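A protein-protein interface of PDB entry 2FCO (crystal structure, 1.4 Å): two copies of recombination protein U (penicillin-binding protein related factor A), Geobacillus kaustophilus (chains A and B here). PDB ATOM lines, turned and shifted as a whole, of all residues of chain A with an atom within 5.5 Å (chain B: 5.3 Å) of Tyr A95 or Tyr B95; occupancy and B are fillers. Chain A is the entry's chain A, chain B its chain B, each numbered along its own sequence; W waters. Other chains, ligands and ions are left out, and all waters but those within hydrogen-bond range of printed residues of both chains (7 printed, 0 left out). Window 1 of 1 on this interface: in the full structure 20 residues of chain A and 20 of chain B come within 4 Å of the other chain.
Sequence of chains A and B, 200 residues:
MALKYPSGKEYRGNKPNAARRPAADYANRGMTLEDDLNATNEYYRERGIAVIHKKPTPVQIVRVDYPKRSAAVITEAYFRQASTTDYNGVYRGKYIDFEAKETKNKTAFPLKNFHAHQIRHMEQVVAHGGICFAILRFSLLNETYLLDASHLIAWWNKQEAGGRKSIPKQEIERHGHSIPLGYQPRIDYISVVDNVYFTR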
ATOM      1  N   VAL A  51     -29.225  -6.347  -8.385  1.00  0.00           N
ATOM      2  CA  VAL A  51     -27.977  -5.586  -8.372  1.00  0.00           C
ATOM      3  C   VAL A  51     -26.945  -6.350  -9.186  1.00  0.00           C
ATOM      4  O   VAL A  51     -26.290  -7.272  -8.694  1.00  0.00           O
ATOM      5  CB  VAL A  51     -27.436  -5.362  -6.941  1.00  0.00           C
ATOM      6  CG1 VAL A  51     -26.200  -4.469  -6.991  1.00  0.00           C
ATOM      7  CG2 VAL A  51     -28.502  -4.715  -6.080  1.00  0.00           C
ATOM      8  N   LYS A  55     -18.217  -6.108 -15.098  1.00  0.00           N
ATOM      9  CA  LYS A  55     -16.888  -5.956 -14.528  1.00  0.00           C
ATOM     10  C   LYS A  55     -16.008  -5.122 -15.447  1.00  0.00           C
ATOM     11  O   LYS A  55     -16.117  -5.211 -16.667  1.00  0.00           O
ATOM     12  CB  LYS A  55     -16.251  -7.326 -14.312  1.00  0.00           C
ATOM     13  CG  LYS A  55     -16.946  -8.150 -13.243  1.00  0.00           C
ATOM     14  CD  LYS A  55     -16.331  -9.524 -13.129  1.00  0.00           C
ATOM     15  CE  LYS A  55     -16.954 -10.303 -11.980  1.00  0.00           C
ATOM     16  NZ  LYS A  55     -16.365 -11.665 -11.870  1.00  0.00           N
ATOM     17  N   ASN A  88     -22.049 -10.104 -13.313  1.00  0.00           N
ATOM     18  CA  ASN A  88     -22.493 -10.907 -12.188  1.00  0.00           C
ATOM     19  C   ASN A  88     -23.171 -10.026 -11.155  1.00  0.00           C
ATOM     20  O   ASN A  88     -23.133  -8.794 -11.246  1.00  0.00           O
ATOM     21  CB  ASN A  88     -21.358 -11.785 -11.601  1.00  0.00           C
ATOM     22  CG  ASN A  88     -20.367 -11.026 -10.738  1.00  0.00           C
ATOM     23  OD1 ASN A  88     -20.384  -9.796 -10.652  1.00  0.00           O
ATOM     24  ND2 ASN A  88     -19.477 -11.783 -10.090  1.00  0.00           N
ATOM     25  N   GLY A  89     -23.837 -10.657 -10.202  1.00  0.00           N
ATOM     26  CA  GLY A  89     -24.542  -9.900  -9.189  1.00  0.00           C
ATOM     27  C   GLY A  89     -25.520 -10.791  -8.465  1.00  0.00           C
ATOM     28  O   GLY A  89     -25.377 -12.018  -8.478  1.00  0.00           O
ATOM     29  N   VAL A  90     -26.528 -10.180  -7.854  1.00  0.00           N
ATOM     30  CA  VAL A  90     -27.505 -10.935  -7.090  1.00  0.00           C
ATOM     31  C   VAL A  90     -28.950 -10.568  -7.410  1.00  0.00           C
ATOM     32  O   VAL A  90     -29.273  -9.413  -7.715  1.00  0.00           O
ATOM     33  CB  VAL A  90     -27.240 -10.758  -5.564  1.00  0.00           C
ATOM     34  CG1 VAL A  90     -27.354  -9.292  -5.178  1.00  0.00           C
ATOM     35  CG2 VAL A  90     -28.200 -11.616  -4.751  1.00  0.00           C
ATOM     36  N   TYR A  91     -29.802 -11.583  -7.362  1.00  0.00           N
ATOM     37  CA  TYR A  91     -31.229 -11.438  -7.608  1.00  0.00           C
ATOM     38  C   TYR A  91     -31.935 -12.487  -6.758  1.00  0.00           C
ATOM     39  O   TYR A  91     -31.636 -13.676  -6.853  1.00  0.00           O
ATOM     40  CB  TYR A  91     -31.565 -11.668  -9.085  1.00  0.00           C
ATOM     41  CG  TYR A  91     -33.055 -11.626  -9.363  1.00  0.00           C
ATOM     42  CD1 TYR A  91     -33.786 -10.457  -9.159  1.00  0.00           C
ATOM     43  CD2 TYR A  91     -33.735 -12.762  -9.801  1.00  0.00           C
ATOM     44  CE1 TYR A  91     -35.165 -10.420  -9.384  1.00  0.00           C
ATOM     45  CE2 TYR A  91     -35.116 -12.737 -10.031  1.00  0.00           C
ATOM     46  CZ  TYR A  91     -35.820 -11.560  -9.819  1.00  0.00           C
ATOM     47  OH  TYR A  91     -37.181 -11.516 -10.043  1.00  0.00           O
ATOM     48  N   GLY A  93     -31.628 -13.389  -3.764  1.00  0.00           N
ATOM     49  CA  GLY A  93     -30.730 -14.212  -2.975  1.00  0.00           C
ATOM     50  C   GLY A  93     -29.875 -15.218  -3.719  1.00  0.00           C
ATOM     51  O   GLY A  93     -29.203 -16.035  -3.089  1.00  0.00           O
ATOM     52  N   LYS A  94     -29.893 -15.173  -5.047  1.00  0.00           N
ATOM     53  CA  LYS A  94     -29.097 -16.099  -5.836  1.00  0.00           C
ATOM     54  C   LYS A  94     -28.016 -15.380  -6.622  1.00  0.00           C
ATOM     55  O   LYS A  94     -28.186 -14.231  -7.040  1.00  0.00           O
ATOM     56  CB  LYS A  94     -29.976 -16.875  -6.821  1.00  0.00           C
ATOM     57  CG  LYS A  94     -31.004 -17.774  -6.166  1.00  0.00           C
ATOM     58  CD  LYS A  94     -31.669 -18.683  -7.187  1.00  0.00           C
ATOM     59  CE  LYS A  94     -32.676 -19.613  -6.523  1.00  0.00           C
ATOM     60  NZ  LYS A  94     -33.311 -20.536  -7.509  1.00  0.00           N
ATOM     61  N   TYR A  95     -26.899 -16.070  -6.814  1.00  0.00           N
ATOM     62  CA  TYR A  95     -25.781 -15.544  -7.584  1.00  0.00           C
ATOM     63  C   TYR A  95     -26.161 -15.603  -9.066  1.00  0.00           C
ATOM     64  O   TYR A  95     -26.576 -16.657  -9.556  1.00  0.00           O
ATOM     65  CB  TYR A  95     -24.547 -16.414  -7.353  1.00  0.00           C
ATOM     66  CG  TYR A  95     -23.343 -15.997  -8.161  1.00  0.00           C
ATOM     67  CD1 TYR A  95     -22.553 -14.929  -7.758  1.00  0.00           C
ATOM     68  CD2 TYR A  95     -22.988 -16.678  -9.325  1.00  0.00           C
ATOM     69  CE1 TYR A  95     -21.439 -14.542  -8.483  1.00  0.00           C
ATOM     70  CE2 TYR A  95     -21.869 -16.299 -10.064  1.00  0.00           C
ATOM     71  CZ  TYR A  95     -21.099 -15.228  -9.635  1.00  0.00           C
ATOM     72  OH  TYR A  95     -19.993 -14.832 -10.347  1.00  0.00           O
ATOM     73  N   ILE A  96     -26.012 -14.480  -9.763  1.00  0.00           N
ATOM     74  CA  ILE A  96     -26.326 -14.390 -11.192  1.00  0.00           C
ATOM     75  C   ILE A  96     -25.021 -14.092 -11.924  1.00  0.00           C
ATOM     76  O   ILE A  96     -24.248 -13.236 -11.496  1.00  0.00           O
ATOM     77  CB  ILE A  96     -27.310 -13.240 -11.482  1.00  0.00           C
ATOM     78  CG1 ILE A  96     -28.516 -13.326 -10.545  1.00  0.00           C
ATOM     79  CG2 ILE A  96     -27.737 -13.286 -12.950  1.00  0.00           C
ATOM     80  CD1 ILE A  96     -29.342 -14.593 -10.695  1.00  0.00           C
ATOM     81  N   ASP A  97     -24.784 -14.776 -13.038  1.00  0.00           N
ATOM     82  CA  ASP A  97     -23.539 -14.591 -13.775  1.00  0.00           C
ATOM     83  C   ASP A  97     -23.807 -14.848 -15.252  1.00  0.00           C
ATOM     84  O   ASP A  97     -24.422 -15.848 -15.607  1.00  0.00           O
ATOM     85  CB  ASP A  97     -22.510 -15.593 -13.219  1.00  0.00           C
ATOM     86  CG  ASP A  97     -21.110 -15.404 -13.780  1.00  0.00           C
ATOM     87  OD1 ASP A  97     -20.919 -15.589 -15.002  1.00  0.00           O
ATOM     88  OD2 ASP A  97     -20.185 -15.089 -12.989  1.00  0.00           O
ATOM     89  N   HIS A 121     -15.093 -20.722 -16.537  1.00  0.00           N
ATOM     90  CA  HIS A 121     -15.669 -19.974 -15.422  1.00  0.00           C
ATOM     91  C   HIS A 121     -17.147 -20.327 -15.271  1.00  0.00           C
ATOM     92  O   HIS A 121     -17.635 -20.531 -14.158  1.00  0.00           O
ATOM     93  CB  HIS A 121     -15.527 -18.471 -15.650  1.00  0.00           C
ATOM     94  CG  HIS A 121     -16.249 -17.641 -14.636  1.00  0.00           C
ATOM     95  ND1 HIS A 121     -15.798 -17.482 -13.343  1.00  0.00           N
ATOM     96  CD2 HIS A 121     -17.407 -16.944 -14.719  1.00  0.00           C
ATOM     97  CE1 HIS A 121     -16.646 -16.722 -12.674  1.00  0.00           C
ATOM     98  NE2 HIS A 121     -17.632 -16.383 -13.486  1.00  0.00           N
ATOM     99  N   VAL A 125     -19.170 -21.787 -12.052  1.00  0.00           N
ATOM    100  CA  VAL A 125     -20.350 -21.156 -11.467  1.00  0.00           C
ATOM    101  C   VAL A 125     -21.507 -22.147 -11.365  1.00  0.00           C
ATOM    102  O   VAL A 125     -22.195 -22.210 -10.343  1.00  0.00           O
ATOM    103  CB  VAL A 125     -20.805 -19.928 -12.301  1.00  0.00           C
ATOM    104  CG1 VAL A 125     -22.147 -19.426 -11.791  1.00  0.00           C
ATOM    105  CG2 VAL A 125     -19.759 -18.824 -12.208  1.00  0.00           C
ATOM    106  N   GLY A 129     -23.655 -23.859  -7.822  1.00  0.00           N
ATOM    107  CA  GLY A 129     -25.050 -23.485  -7.645  1.00  0.00           C
ATOM    108  C   GLY A 129     -25.535 -22.137  -8.127  1.00  0.00           C
ATOM    109  O   GLY A 129     -26.646 -21.728  -7.787  1.00  0.00           O
ATOM    110  N   GLY A 130     -24.728 -21.444  -8.917  1.00  0.00           N
ATOM    111  CA  GLY A 130     -25.159 -20.147  -9.399  1.00  0.00           C
ATOM    112  C   GLY A 130     -26.016 -20.243 -10.645  1.00  0.00           C
ATOM    113  O   GLY A 130     -26.053 -21.283 -11.304  1.00  0.00           O
ATOM    114  N   ILE A 131     -26.734 -19.163 -10.942  1.00  0.00           N
ATOM    115  CA  ILE A 131     -27.557 -19.085 -12.145  1.00  0.00           C
ATOM    116  C   ILE A 131     -26.595 -18.500 -13.171  1.00  0.00           C
ATOM    117  O   ILE A 131     -26.086 -17.390 -13.002  1.00  0.00           O
ATOM    118  CB  ILE A 131     -28.762 -18.146 -11.936  1.00  0.00           C
ATOM    119  CG1 ILE A 131     -29.724 -18.767 -10.917  1.00  0.00           C
ATOM    120  CG2 ILE A 131     -29.464 -17.887 -13.270  1.00  0.00           C
ATOM    121  CD1 ILE A 131     -30.864 -17.849 -10.507  1.00  0.00           C
ATOM    122  N   CYS A 132     -26.337 -19.250 -14.234  1.00  0.00           N
ATOM    123  CA  CYS A 132     -25.377 -18.815 -15.233  1.00  0.00           C
ATOM    124  C   CYS A 132     -25.938 -19.011 -16.628  1.00  0.00           C
ATOM    125  O   CYS A 132     -26.492 -20.063 -16.939  1.00  0.00           O
ATOM    126  CB  CYS A 132     -24.084 -19.621 -15.052  1.00  0.00           C
ATOM    127  SG  CYS A 132     -22.662 -19.018 -15.961  1.00  0.00           S
ATOM    128  N   VAL B  51     -15.864 -19.613  -5.758  1.00  0.00           N
ATOM    129  CA  VAL B  51     -15.335 -18.911  -6.919  1.00  0.00           C
ATOM    130  C   VAL B  51     -15.512 -17.426  -6.670  1.00  0.00           C
ATOM    131  O   VAL B  51     -16.541 -16.833  -7.003  1.00  0.00           O
ATOM    132  CB  VAL B  51     -16.061 -19.324  -8.213  1.00  0.00           C
ATOM    133  CG1 VAL B  51     -15.360 -18.716  -9.424  1.00  0.00           C
ATOM    134  CG2 VAL B  51     -16.071 -20.843  -8.327  1.00  0.00           C
ATOM    135  N   LYS B  55     -12.353  -7.733  -8.415  1.00  0.00           N
ATOM    136  CA  LYS B  55     -12.710  -7.094  -9.676  1.00  0.00           C
ATOM    137  C   LYS B  55     -11.552  -6.293 -10.246  1.00  0.00           C
ATOM    138  O   LYS B  55     -10.766  -5.710  -9.501  1.00  0.00           O
ATOM    139  CB  LYS B  55     -13.913  -6.167  -9.480  1.00  0.00           C
ATOM    140  CG  LYS B  55     -15.211  -6.898  -9.196  1.00  0.00           C
ATOM    141  CD  LYS B  55     -16.376  -5.931  -9.055  1.00  0.00           C
ATOM    142  CE  LYS B  55     -17.698  -6.681  -8.962  1.00  0.00           C
ATOM    143  NZ  LYS B  55     -18.872  -5.761  -8.891  1.00  0.00           N
ATOM    144  N   ASN B  88     -16.171 -10.178  -5.164  1.00  0.00           N
ATOM    145  CA  ASN B  88     -17.454 -10.853  -5.219  1.00  0.00           C
ATOM    146  C   ASN B  88     -17.329 -12.203  -5.905  1.00  0.00           C
ATOM    147  O   ASN B  88     -16.312 -12.514  -6.528  1.00  0.00           O
ATOM    148  CB  ASN B  88     -18.562  -9.965  -5.842  1.00  0.00           C
ATOM    149  CG  ASN B  88     -18.544  -9.914  -7.368  1.00  0.00           C
ATOM    150  OD1 ASN B  88     -17.737 -10.550  -8.039  1.00  0.00           O
ATOM    151  ND2 ASN B  88     -19.478  -9.140  -7.919  1.00  0.00           N
ATOM    152  N   GLY B  89     -18.350 -13.026  -5.740  1.00  0.00           N
ATOM    153  CA  GLY B  89     -18.313 -14.341  -6.339  1.00  0.00           C
ATOM    154  C   GLY B  89     -19.433 -15.201  -5.814  1.00  0.00           C
ATOM    155  O   GLY B  89     -20.404 -14.699  -5.237  1.00  0.00           O
ATOM    156  N   VAL B  90     -19.287 -16.510  -5.993  1.00  0.00           N
ATOM    157  CA  VAL B  90     -20.314 -17.446  -5.580  1.00  0.00           C
ATOM    158  C   VAL B  90     -19.833 -18.508  -4.591  1.00  0.00           C
ATOM    159  O   VAL B  90     -18.703 -18.996  -4.666  1.00  0.00           O
ATOM    160  CB  VAL B  90     -20.931 -18.141  -6.833  1.00  0.00           C
ATOM    161  CG1 VAL B  90     -19.861 -18.937  -7.577  1.00  0.00           C
ATOM    162  CG2 VAL B  90     -22.100 -19.036  -6.423  1.00  0.00           C
ATOM    163  N   TYR B  91     -20.706 -18.837  -3.646  1.00  0.00           N
ATOM    164  CA  TYR B  91     -20.428 -19.862  -2.652  1.00  0.00           C
ATOM    165  C   TYR B  91     -21.772 -20.461  -2.257  1.00  0.00           C
ATOM    166  O   TYR B  91     -22.665 -19.745  -1.810  1.00  0.00           O
ATOM    167  CB  TYR B  91     -19.741 -19.260  -1.421  1.00  0.00           C
ATOM    168  CG  TYR B  91     -19.466 -20.281  -0.341  1.00  0.00           C
ATOM    169  CD1 TYR B  91     -18.595 -21.346  -0.572  1.00  0.00           C
ATOM    170  CD2 TYR B  91     -20.099 -20.200   0.896  1.00  0.00           C
ATOM    171  CE1 TYR B  91     -18.363 -22.309   0.403  1.00  0.00           C
ATOM    172  CE2 TYR B  91     -19.874 -21.161   1.886  1.00  0.00           C
ATOM    173  CZ  TYR B  91     -19.004 -22.211   1.624  1.00  0.00           C
ATOM    174  OH  TYR B  91     -18.772 -23.172   2.577  1.00  0.00           O
ATOM    175  N   GLY B  93     -24.225 -21.384  -3.992  1.00  0.00           N
ATOM    176  CA  GLY B  93     -25.301 -20.749  -4.736  1.00  0.00           C
ATOM    177  C   GLY B  93     -25.608 -19.311  -4.373  1.00  0.00           C
ATOM    178  O   GLY B  93     -26.397 -18.645  -5.054  1.00  0.00           O
ATOM    179  N   LYS B  94     -24.984 -18.820  -3.308  1.00  0.00           N
ATOM    180  CA  LYS B  94     -25.227 -17.452  -2.864  1.00  0.00           C
ATOM    181  C   LYS B  94     -24.206 -16.476  -3.427  1.00  0.00           C
ATOM    182  O   LYS B  94     -23.098 -16.860  -3.809  1.00  0.00           O
ATOM    183  CB  LYS B  94     -25.192 -17.379  -1.334  1.00  0.00           C
ATOM    184  CG  LYS B  94     -26.034 -18.435  -0.632  1.00  0.00           C
ATOM    185  CD  LYS B  94     -27.514 -18.284  -0.932  1.00  0.00           C
ATOM    186  CE  LYS B  94     -28.114 -17.080  -0.230  1.00  0.00           C
ATOM    187  NZ  LYS B  94     -29.590 -17.021  -0.448  1.00  0.00           N
ATOM    188  N   TYR B  95     -24.599 -15.210  -3.474  1.00  0.00           N
ATOM    189  CA  TYR B  95     -23.742 -14.138  -3.956  1.00  0.00           C
ATOM    190  C   TYR B  95     -22.949 -13.613  -2.760  1.00  0.00           C
ATOM    191  O   TYR B  95     -23.538 -13.186  -1.768  1.00  0.00           O
ATOM    192  CB  TYR B  95     -24.602 -13.004  -4.531  1.00  0.00           C
ATOM    193  CG  TYR B  95     -23.828 -11.769  -4.941  1.00  0.00           C
ATOM    194  CD1 TYR B  95     -23.047 -11.759  -6.097  1.00  0.00           C
ATOM    195  CD2 TYR B  95     -23.876 -10.608  -4.170  1.00  0.00           C
ATOM    196  CE1 TYR B  95     -22.332 -10.622  -6.477  1.00  0.00           C
ATOM    197  CE2 TYR B  95     -23.167  -9.467  -4.539  1.00  0.00           C
ATOM    198  CZ  TYR B  95     -22.396  -9.480  -5.692  1.00  0.00           C
ATOM    199  OH  TYR B  95     -21.678  -8.366  -6.066  1.00  0.00           O
ATOM    200  N   ILE B  96     -21.624 -13.666  -2.854  1.00  0.00           N
ATOM    201  CA  ILE B  96     -20.731 -13.180  -1.799  1.00  0.00           C
ATOM    202  C   ILE B  96     -20.134 -11.870  -2.299  1.00  0.00           C
ATOM    203  O   ILE B  96     -19.712 -11.777  -3.450  1.00  0.00           O
ATOM    204  CB  ILE B  96     -19.582 -14.166  -1.539  1.00  0.00           C
ATOM    205  CG1 ILE B  96     -20.136 -15.572  -1.309  1.00  0.00           C
ATOM    206  CG2 ILE B  96     -18.748 -13.689  -0.350  1.00  0.00           C
ATOM    207  CD1 ILE B  96     -21.127 -15.683  -0.155  1.00  0.00           C
ATOM    208  N   ASP B  97     -20.082 -10.863  -1.434  1.00  0.00           N
ATOM    209  CA  ASP B  97     -19.568  -9.559  -1.831  1.00  0.00           C
ATOM    210  C   ASP B  97     -18.883  -8.912  -0.635  1.00  0.00           C
ATOM    211  O   ASP B  97     -19.451  -8.871   0.454  1.00  0.00           O
ATOM    212  CB  ASP B  97     -20.757  -8.707  -2.305  1.00  0.00           C
ATOM    213  CG  ASP B  97     -20.354  -7.338  -2.826  1.00  0.00           C
ATOM    214  OD1 ASP B  97     -19.838  -6.519  -2.037  1.00  0.00           O
ATOM    215  OD2 ASP B  97     -20.572  -7.073  -4.032  1.00  0.00           O
ATOM    216  N   HIS B 121     -23.629   0.558  -2.521  1.00  0.00           N
ATOM    217  CA  HIS B 121     -23.615  -0.742  -3.186  1.00  0.00           C
ATOM    218  C   HIS B 121     -23.901  -1.846  -2.172  1.00  0.00           C
ATOM    219  O   HIS B 121     -24.701  -2.744  -2.427  1.00  0.00           O
ATOM    220  CB  HIS B 121     -22.251  -0.993  -3.837  1.00  0.00           C
ATOM    221  CG  HIS B 121     -22.073  -2.394  -4.336  1.00  0.00           C
ATOM    222  ND1 HIS B 121     -22.760  -2.892  -5.424  1.00  0.00           N
ATOM    223  CD2 HIS B 121     -21.313  -3.414  -3.872  1.00  0.00           C
ATOM    224  CE1 HIS B 121     -22.429  -4.159  -5.606  1.00  0.00           C
ATOM    225  NE2 HIS B 121     -21.553  -4.499  -4.678  1.00  0.00           N
ATOM    226  N   VAL B 125     -26.826  -4.742  -2.096  1.00  0.00           N
ATOM    227  CA  VAL B 125     -26.544  -6.175  -2.032  1.00  0.00           C
ATOM    228  C   VAL B 125     -27.294  -6.819  -0.868  1.00  0.00           C
ATOM    229  O   VAL B 125     -27.889  -7.886  -1.014  1.00  0.00           O
ATOM    230  CB  VAL B 125     -25.026  -6.445  -1.876  1.00  0.00           C
ATOM    231  CG1 VAL B 125     -24.778  -7.929  -1.639  1.00  0.00           C
ATOM    232  CG2 VAL B 125     -24.290  -5.992  -3.132  1.00  0.00           C
ATOM    233  N   GLY B 129     -30.586  -9.995  -0.749  1.00  0.00           N
ATOM    234  CA  GLY B 129     -30.247 -11.317  -0.259  1.00  0.00           C
ATOM    235  C   GLY B 129     -28.815 -11.781  -0.426  1.00  0.00           C
ATOM    236  O   GLY B 129     -28.530 -12.967  -0.274  1.00  0.00           O
ATOM    237  N   GLY B 130     -27.914 -10.860  -0.735  1.00  0.00           N
ATOM    238  CA  GLY B 130     -26.525 -11.251  -0.880  1.00  0.00           C
ATOM    239  C   GLY B 130     -25.851 -11.299   0.480  1.00  0.00           C
ATOM    240  O   GLY B 130     -26.362 -10.736   1.449  1.00  0.00           O
ATOM    241  N   ILE B 131     -24.728 -12.006   0.557  1.00  0.00           N
ATOM    242  CA  ILE B 131     -23.942 -12.095   1.788  1.00  0.00           C
ATOM    243  C   ILE B 131     -22.884 -11.026   1.563  1.00  0.00           C
ATOM    244  O   ILE B 131     -22.035 -11.158   0.682  1.00  0.00           O
ATOM    245  CB  ILE B 131     -23.300 -13.482   1.929  1.00  0.00           C
ATOM    246  CG1 ILE B 131     -24.398 -14.518   2.192  1.00  0.00           C
ATOM    247  CG2 ILE B 131     -22.283 -13.481   3.069  1.00  0.00           C
ATOM    248  CD1 ILE B 131     -23.915 -15.948   2.220  1.00  0.00           C
ATOM    249  N   CYS B 132     -22.948  -9.964   2.356  1.00  0.00           N
ATOM    250  CA  CYS B 132     -22.053  -8.830   2.176  1.00  0.00           C
ATOM    251  C   CYS B 132     -21.382  -8.438   3.483  1.00  0.00           C
ATOM    252  O   CYS B 132     -22.043  -8.317   4.511  1.00  0.00           O
ATOM    253  CB  CYS B 132     -22.884  -7.668   1.627  1.00  0.00           C
ATOM    254  SG  CYS B 132     -21.969  -6.259   1.032  1.00  0.00           S
HETATM  255  O   HOH W   1     -21.516  -7.106  -9.364  1.00  0.00           O
HETATM  256  O   HOH W   2     -27.073 -14.567  -2.194  1.00  0.00           O
HETATM  257  O   HOH W   3     -30.237 -18.748  -2.354  1.00  0.00           O
HETATM  258  O   HOH W   4     -19.755  -7.378 -11.860  1.00  0.00           O
HETATM  259  O   HOH W   5     -17.409 -15.664  -9.511  1.00  0.00           O
HETATM  260  O   HOH W   6     -23.516  -6.725  -7.702  1.00  0.00           O
HETATM  261  O   HOH W   7     -16.418 -13.056  -9.470  1.00  0.00           O
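The side-chain amide oxygen (OD1) of Asn A88 lies within hydrogen-bond range of the side-chain amide nitrogen (ND2) of Asn B88 (3.0 Å). The side-chain amino group (NZ) of Lys B94 sits at hydrogen-bond distance from the backbone carbonyl oxygen (O) of Gly A93. The backbone NH (N) of Tyr A95 is in hydrogen-bond range of the backbone carbonyl oxygen (O) of Gly B93 (3.2 Å).
Of the 17 printed residues of chain B, 7 touch a printed residue of chain A. Printed residues of chain A that touch a printed residue of chain B: Asn A88, Gly A89, Val A90, Gly A93, Lys A94, Tyr A95 and Gly A129. Among the printed residues, 12 pairs touch across the chains.
Gly A89 touches Tyr B95, and with the chains exchanged Tyr A95 touches Gly B89. Gly A93 touches Gly B129, and with the chains exchanged Gly A129 touches Gly B93. Tyr A95 touches Lys B94, but with the chains exchanged Lys A94 does not touch Tyr B95 (4.5 Å). Tyr A95 touches its own counterpart, Tyr B95. 17 positions are printed for both chains.
Of the printed residues of chain B, Asn A88 touches Asn B88 (3.0 Å). Tyr A95 touches just these residues of chain B: Gly B89, Val B90, Gly B93, Lys B94 and Tyr B95. His A121 touches none of the printed residues of chain B. Val A125 touches none of the printed residues of chain B. Of the printed residues of chain A, Val B90 touches Tyr A95. Tyr B95 touches just these residues of chain A: Gly A89, Val A90 and Tyr A95. The nearest printed residue of chain B that does not touch Val A90 is Gly B130 (4.1 Å).
Water W3 lies within hydrogen-bond range of the side-chain amino group (NZ) of Lys B94 (2.7 Å) and the backbone carbonyl oxygen (O) of Gly A93 (3.0 Å). Water W2 lies within hydrogen-bond range of the backbone carbonyl oxygen (O) of Gly A93 (2.7 Å), the backbone NH (N) of Tyr B95 (2.9 Å) and the backbone carbonyl oxygen (O) of Gly B129 (2.9 Å). Water W7 lies within hydrogen-bond range of the side-chain amino group of Lys A55, the backbone carbonyl oxygen of Asn B88 and the side-chain amide nitrogen of Asn A88. Water W4 lies within hydrogen-bond range of the side-chain amide oxygen (OD1) of Asn A88 (2.8 Å) and the side-chain amino group (NZ) of Lys B55 (3.5 Å). Water W6 lies within hydrogen-bond range of the side-chain hydroxyl of Tyr B95 and the backbone carbonyl oxygen of Val A51. Water W1 lies within hydrogen-bond range of O of Asn A88 (3.0 Å), NZ of Lys B55 (3.0 Å) and ND2 of Asn B88 (3.2 Å).
Among the printed residues, merely in contact across the chains: Gly A89 with Tyr B95, Val A90 with Tyr B95, Gly A93 with Gly B129, Lys A94 with Gly B93, Tyr A95 with Gly B89, Tyr A95 with Val B90, Tyr A95 with Lys B94, Tyr A95 with Tyr B95 and Gly A129 with Gly B93.
The backbone NH (N) of Val A90 lies within hydrogen-bond range of the backbone carbonyl oxygen (O) of Val A51 (3.0 Å). N of Ile A96 lies within hydrogen-bond range of O of Gly A89 (2.8 Å). The backbone NH of Val B90 is in hydrogen-bond range of the backbone carbonyl oxygen of Val B51. OH of Tyr B95 lies within hydrogen-bond range of ND2 of Asn B88 (3.0 Å). The backbone carbonyl oxygen of Gly B89 is in hydrogen-bond range of the backbone NH of Ile B96. The backbone carbonyl oxygen (O) of Tyr B95 sits at hydrogen-bond distance from the backbone NH (N) of Ile B131, 2.9 Å away.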
